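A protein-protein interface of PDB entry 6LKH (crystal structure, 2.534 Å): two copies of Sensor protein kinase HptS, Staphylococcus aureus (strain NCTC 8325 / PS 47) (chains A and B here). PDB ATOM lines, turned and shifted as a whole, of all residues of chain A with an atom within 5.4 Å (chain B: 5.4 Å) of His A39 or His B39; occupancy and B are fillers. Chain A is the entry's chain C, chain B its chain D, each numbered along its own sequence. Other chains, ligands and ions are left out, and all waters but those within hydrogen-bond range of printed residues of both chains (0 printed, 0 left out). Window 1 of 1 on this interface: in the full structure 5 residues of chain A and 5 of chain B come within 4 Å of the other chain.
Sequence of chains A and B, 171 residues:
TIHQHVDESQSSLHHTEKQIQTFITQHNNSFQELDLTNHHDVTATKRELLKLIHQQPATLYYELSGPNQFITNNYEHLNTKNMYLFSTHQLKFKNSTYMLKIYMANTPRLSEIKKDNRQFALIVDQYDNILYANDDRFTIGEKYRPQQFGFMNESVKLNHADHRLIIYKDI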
ATOM      1  N   THR A  37       6.504 -26.041  25.994  1.00  0.00           N
ATOM      2  CA  THR A  37       7.827 -26.221  26.583  1.00  0.00           C
ATOM      3  C   THR A  37       8.727 -27.088  25.715  1.00  0.00           C
ATOM      4  O   THR A  37       9.917 -27.232  26.021  1.00  0.00           O
ATOM      5  CB  THR A  37       7.721 -26.864  27.972  1.00  0.00           C
ATOM      6  OG1 THR A  37       7.406 -28.255  27.833  1.00  0.00           O
ATOM      7  CG2 THR A  37       6.647 -26.185  28.814  1.00  0.00           C
ATOM      8  N   ASN A  38       8.180 -27.659  24.647  1.00  0.00           N
ATOM      9  CA  ASN A  38       8.882 -28.577  23.760  1.00  0.00           C
ATOM     10  C   ASN A  38       9.179 -27.851  22.454  1.00  0.00           C
ATOM     11  O   ASN A  38       8.262 -27.355  21.791  1.00  0.00           O
ATOM     12  CB  ASN A  38       8.034 -29.828  23.527  1.00  0.00           C
ATOM     13  CG  ASN A  38       8.423 -30.582  22.273  1.00  0.00           C
ATOM     14  OD1 ASN A  38       9.594 -30.637  21.899  1.00  0.00           O
ATOM     15  ND2 ASN A  38       7.432 -31.171  21.613  1.00  0.00           N
ATOM     16  N   HIS A  39      10.459 -27.791  22.087  1.00  0.00           N
ATOM     17  CA  HIS A  39      10.895 -26.935  20.993  1.00  0.00           C
ATOM     18  C   HIS A  39      10.450 -27.433  19.622  1.00  0.00           C
ATOM     19  O   HIS A  39      10.560 -26.678  18.650  1.00  0.00           O
ATOM     20  CB  HIS A  39      12.415 -26.787  21.048  1.00  0.00           C
ATOM     21  CG  HIS A  39      12.901 -26.147  22.311  1.00  0.00           C
ATOM     22  ND1 HIS A  39      12.606 -24.842  22.640  1.00  0.00           N
ATOM     23  CD2 HIS A  39      13.643 -26.634  23.333  1.00  0.00           C
ATOM     24  CE1 HIS A  39      13.154 -24.548  23.806  1.00  0.00           C
ATOM     25  NE2 HIS A  39      13.788 -25.618  24.249  1.00  0.00           N
ATOM     26  N   HIS A  40       9.952 -28.669  19.516  1.00  0.00           N
ATOM     27  CA  HIS A  40       9.362 -29.123  18.259  1.00  0.00           C
ATOM     28  C   HIS A  40       7.933 -28.617  18.104  1.00  0.00           C
ATOM     29  O   HIS A  40       7.488 -28.329  16.986  1.00  0.00           O
ATOM     30  CB  HIS A  40       9.381 -30.652  18.176  1.00  0.00           C
ATOM     31  CG  HIS A  40      10.748 -31.235  17.999  1.00  0.00           C
ATOM     32  ND1 HIS A  40      11.256 -31.578  16.764  1.00  0.00           N
ATOM     33  CD2 HIS A  40      11.710 -31.544  18.900  1.00  0.00           C
ATOM     34  CE1 HIS A  40      12.474 -32.067  16.912  1.00  0.00           C
ATOM     35  NE2 HIS A  40      12.774 -32.059  18.198  1.00  0.00           N
ATOM     36  N   ASP A  41       7.194 -28.511  19.210  1.00  0.00           N
ATOM     37  CA  ASP A  41       5.819 -28.034  19.147  1.00  0.00           C
ATOM     38  C   ASP A  41       5.748 -26.516  19.034  1.00  0.00           C
ATOM     39  O   ASP A  41       4.801 -25.985  18.442  1.00  0.00           O
ATOM     40  CB  ASP A  41       5.042 -28.509  20.376  1.00  0.00           C
ATOM     41  CG  ASP A  41       4.848 -30.016  20.401  1.00  0.00           C
ATOM     42  OD1 ASP A  41       5.289 -30.696  19.448  1.00  0.00           O
ATOM     43  OD2 ASP A  41       4.254 -30.524  21.376  1.00  0.00           O
ATOM     44  N   VAL A  42       6.728 -25.802  19.591  1.00  0.00           N
ATOM     45  CA  VAL A  42       6.801 -24.358  19.390  1.00  0.00           C
ATOM     46  C   VAL A  42       6.961 -24.049  17.907  1.00  0.00           C
ATOM     47  O   VAL A  42       6.266 -23.191  17.351  1.00  0.00           O
ATOM     48  CB  VAL A  42       7.945 -23.761  20.230  1.00  0.00           C
ATOM     49  CG1 VAL A  42       8.256 -22.326  19.817  1.00  0.00           C
ATOM     50  CG2 VAL A  42       7.579 -23.810  21.704  1.00  0.00           C
ATOM     51  N   THR A  43       7.874 -24.758  17.240  1.00  0.00           N
ATOM     52  CA  THR A  43       8.026 -24.591  15.800  1.00  0.00           C
ATOM     53  C   THR A  43       6.717 -24.884  15.079  1.00  0.00           C
ATOM     54  O   THR A  43       6.386 -24.231  14.082  1.00  0.00           O
ATOM     55  CB  THR A  43       9.147 -25.500  15.291  1.00  0.00           C
ATOM     56  OG1 THR A  43      10.402 -25.037  15.807  1.00  0.00           O
ATOM     57  CG2 THR A  43       9.209 -25.512  13.763  1.00  0.00           C
ATOM     58  N   LYS A  46       4.555 -21.707  15.537  1.00  0.00           N
ATOM     59  CA  LYS A  46       5.066 -20.588  14.752  1.00  0.00           C
ATOM     60  C   LYS A  46       4.772 -20.777  13.273  1.00  0.00           C
ATOM     61  O   LYS A  46       4.362 -19.833  12.588  1.00  0.00           O
ATOM     62  CB  LYS A  46       6.569 -20.427  14.976  1.00  0.00           C
ATOM     63  CG  LYS A  46       6.935 -19.835  16.318  1.00  0.00           C
ATOM     64  CD  LYS A  46       8.437 -19.852  16.539  1.00  0.00           C
ATOM     65  CE  LYS A  46       8.805 -19.249  17.877  1.00  0.00           C
ATOM     66  NZ  LYS A  46      10.276 -19.184  18.047  1.00  0.00           N
ATOM     67  N   THR B  37      16.544 -16.834  23.333  1.00  0.00           N
ATOM     68  CA  THR B  37      15.315 -16.897  22.551  1.00  0.00           C
ATOM     69  C   THR B  37      15.497 -17.704  21.272  1.00  0.00           C
ATOM     70  O   THR B  37      14.542 -17.856  20.502  1.00  0.00           O
ATOM     71  CB  THR B  37      14.830 -15.482  22.205  1.00  0.00           C
ATOM     72  OG1 THR B  37      15.715 -14.884  21.251  1.00  0.00           O
ATOM     73  CG2 THR B  37      14.772 -14.610  23.458  1.00  0.00           C
ATOM     74  N   ASN B  38      16.701 -18.226  21.042  1.00  0.00           N
ATOM     75  CA  ASN B  38      17.037 -19.019  19.866  1.00  0.00           C
ATOM     76  C   ASN B  38      17.139 -20.479  20.288  1.00  0.00           C
ATOM     77  O   ASN B  38      17.912 -20.816  21.193  1.00  0.00           O
ATOM     78  CB  ASN B  38      18.350 -18.527  19.256  1.00  0.00           C
ATOM     79  CG  ASN B  38      18.748 -19.297  18.013  1.00  0.00           C
ATOM     80  OD1 ASN B  38      18.270 -20.403  17.766  1.00  0.00           O
ATOM     81  ND2 ASN B  38      19.643 -18.713  17.226  1.00  0.00           N
ATOM     82  N   HIS B  39      16.370 -21.345  19.625  1.00  0.00           N
ATOM     83  CA  HIS B  39      16.240 -22.725  20.078  1.00  0.00           C
ATOM     84  C   HIS B  39      17.510 -23.539  19.865  1.00  0.00           C
ATOM     85  O   HIS B  39      17.653 -24.602  20.480  1.00  0.00           O
ATOM     86  CB  HIS B  39      15.056 -23.388  19.374  1.00  0.00           C
ATOM     87  CG  HIS B  39      13.738 -22.746  19.685  1.00  0.00           C
ATOM     88  ND1 HIS B  39      13.201 -22.735  20.953  1.00  0.00           N
ATOM     89  CD2 HIS B  39      12.854 -22.090  18.896  1.00  0.00           C
ATOM     90  CE1 HIS B  39      12.041 -22.104  20.933  1.00  0.00           C
ATOM     91  NE2 HIS B  39      11.807 -21.701  19.697  1.00  0.00           N
ATOM     92  N   HIS B  40      18.435 -23.075  19.019  1.00  0.00           N
ATOM     93  CA  HIS B  40      19.721 -23.757  18.879  1.00  0.00           C
ATOM     94  C   HIS B  40      20.653 -23.411  20.032  1.00  0.00           C
ATOM     95  O   HIS B  40      21.443 -24.256  20.471  1.00  0.00           O
ATOM     96  CB  HIS B  40      20.381 -23.394  17.547  1.00  0.00           C
ATOM     97  CG  HIS B  40      19.908 -24.220  16.393  1.00  0.00           C
ATOM     98  ND1 HIS B  40      20.553 -25.371  15.991  1.00  0.00           N
ATOM     99  CD2 HIS B  40      18.855 -24.066  15.555  1.00  0.00           C
ATOM    100  CE1 HIS B  40      19.916 -25.890  14.957  1.00  0.00           C
ATOM    101  NE2 HIS B  40      18.884 -25.116  14.671  1.00  0.00           N
ATOM    102  N   ASP B  41      20.579 -22.174  20.526  1.00  0.00           N
ATOM    103  CA  ASP B  41      21.415 -21.758  21.643  1.00  0.00           C
ATOM    104  C   ASP B  41      20.871 -22.261  22.974  1.00  0.00           C
ATOM    105  O   ASP B  41      21.650 -22.538  23.892  1.00  0.00           O
ATOM    106  CB  ASP B  41      21.538 -20.235  21.663  1.00  0.00           C
ATOM    107  CG  ASP B  41      22.238 -19.690  20.432  1.00  0.00           C
ATOM    108  OD1 ASP B  41      22.693 -20.499  19.593  1.00  0.00           O
ATOM    109  OD2 ASP B  41      22.334 -18.451  20.300  1.00  0.00           O
ATOM    110  N   VAL B  42      19.548 -22.386  23.100  1.00  0.00           N
ATOM    111  CA  VAL B  42      18.968 -22.972  24.305  1.00  0.00           C
ATOM    112  C   VAL B  42      19.391 -24.429  24.431  1.00  0.00           C
ATOM    113  O   VAL B  42      19.769 -24.895  25.511  1.00  0.00           O
ATOM    114  CB  VAL B  42      17.436 -22.824  24.289  1.00  0.00           C
ATOM    115  CG1 VAL B  42      16.786 -23.689  25.363  1.00  0.00           C
ATOM    116  CG2 VAL B  42      17.054 -21.370  24.489  1.00  0.00           C
ATOM    117  N   THR B  43      19.327 -25.174  23.323  1.00  0.00           N
ATOM    118  CA  THR B  43      19.821 -26.547  23.329  1.00  0.00           C
ATOM    119  C   THR B  43      21.280 -26.595  23.768  1.00  0.00           C
ATOM    120  O   THR B  43      21.689 -27.507  24.497  1.00  0.00           O
ATOM    121  CB  THR B  43      19.653 -27.178  21.942  1.00  0.00           C
ATOM    122  OG1 THR B  43      18.262 -27.372  21.661  1.00  0.00           O
ATOM    123  CG2 THR B  43      20.357 -28.531  21.859  1.00  0.00           C
ATOM    124  N   ALA B  44      22.080 -25.617  23.338  1.00  0.00           N
ATOM    125  CA  ALA B  44      23.486 -25.595  23.721  1.00  0.00           C
ATOM    126  C   ALA B  44      23.660 -25.353  25.216  1.00  0.00           C
ATOM    127  O   ALA B  44      24.606 -25.874  25.818  1.00  0.00           O
ATOM    128  CB  ALA B  44      24.227 -24.526  22.918  1.00  0.00           C
ATOM    129  N   LYS B  46      21.342 -26.216  27.628  1.00  0.00           N
ATOM    130  CA  LYS B  46      20.882 -27.421  28.311  1.00  0.00           C
ATOM    131  C   LYS B  46      21.937 -28.516  28.266  1.00  0.00           C
ATOM    132  O   LYS B  46      22.191 -29.184  29.274  1.00  0.00           O
ATOM    133  CB  LYS B  46      19.578 -27.914  27.683  1.00  0.00           C
ATOM    134  CG  LYS B  46      18.361 -27.080  28.031  1.00  0.00           C
ATOM    135  CD  LYS B  46      17.145 -27.515  27.234  1.00  0.00           C
ATOM    136  CE  LYS B  46      15.922 -26.700  27.608  1.00  0.00           C
ATOM    137  NZ  LYS B  46      14.702 -27.165  26.892  1.00  0.00           N
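A ring nitrogen (ND1) of His B39 is in hydrogen-bond range of a ring nitrogen (ND1) of His A39 (2.8 Å).
The side-chain amino group (NZ) of Lys A46 lies within hydrogen-bond range of a ring nitrogen (NE2) of His B39 (3.4 Å).
The side-chain amino group (NZ) of Lys B46 lies within hydrogen-bond range of a ring nitrogen (NE2) of His A39, 3.2 Å away.
The backbone carbonyl oxygen (O) of His B39 sits at hydrogen-bond distance from the side-chain hydroxyl (OG1) of Thr B43 (3.1 Å).
O of His A39 sits at hydrogen-bond distance from OG1 of Thr A43 (3.3 Å).
Among the printed residues, merely in contact across the chains: His A39 with Val B42 (3.7 Å) and Val A42 with His B39 (3.6 Å).
Of chain B, only His B39 (2.8 Å), Val B42 (3.7 Å) and Lys B46 (3.2 Å) come within 4 Å of His A39.
Of the printed residues of chain B, Lys A46 touches His B39.
Of the printed residues of chain A, Val B42 touches His A39.
Printed residues of chain B within 4 Å of Val A42: His B39 (3.6 Å).
Of the printed residues of chain A, Lys B46 touches His A39 (3.2 Å).
The nearest residue of chain B that does not touch His A39 is Thr B43 (5.0 Å).
Printed residues of chain B that touch a printed residue of chain A: His B39, Val B42 and Lys B46.
Along chain B the printed residues that touch a printed residue of chain A span positions 39 to 46.
Of the 8 printed residues of chain A, 3 touch a printed residue of chain B.
Hydrophobic or aromatic side chains of chain A that line the printed part of chain B: His A39 and Val A42.
Along chain A the printed residues that touch a printed residue of chain B span positions 39 to 46.
Among the printed residues, 5 pairs touch across the chains.
Among the printed residues, no Asp or Glu carboxylate lies within 4 Å of a Lys or Arg side-chain nitrogen of the other chain.
His A39 touches its own counterpart, His B39.
His A39 touches Val B42, and with the chains exchanged Val A42 touches His B39.
His A39 touches Lys B46, and with the chains exchanged Lys A46 touches His B39.
8 positions are printed for both chains.
Of the 5 pairs that touch across the chains among the printed residues, 5 have their exchanged pair printed and touching as well.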
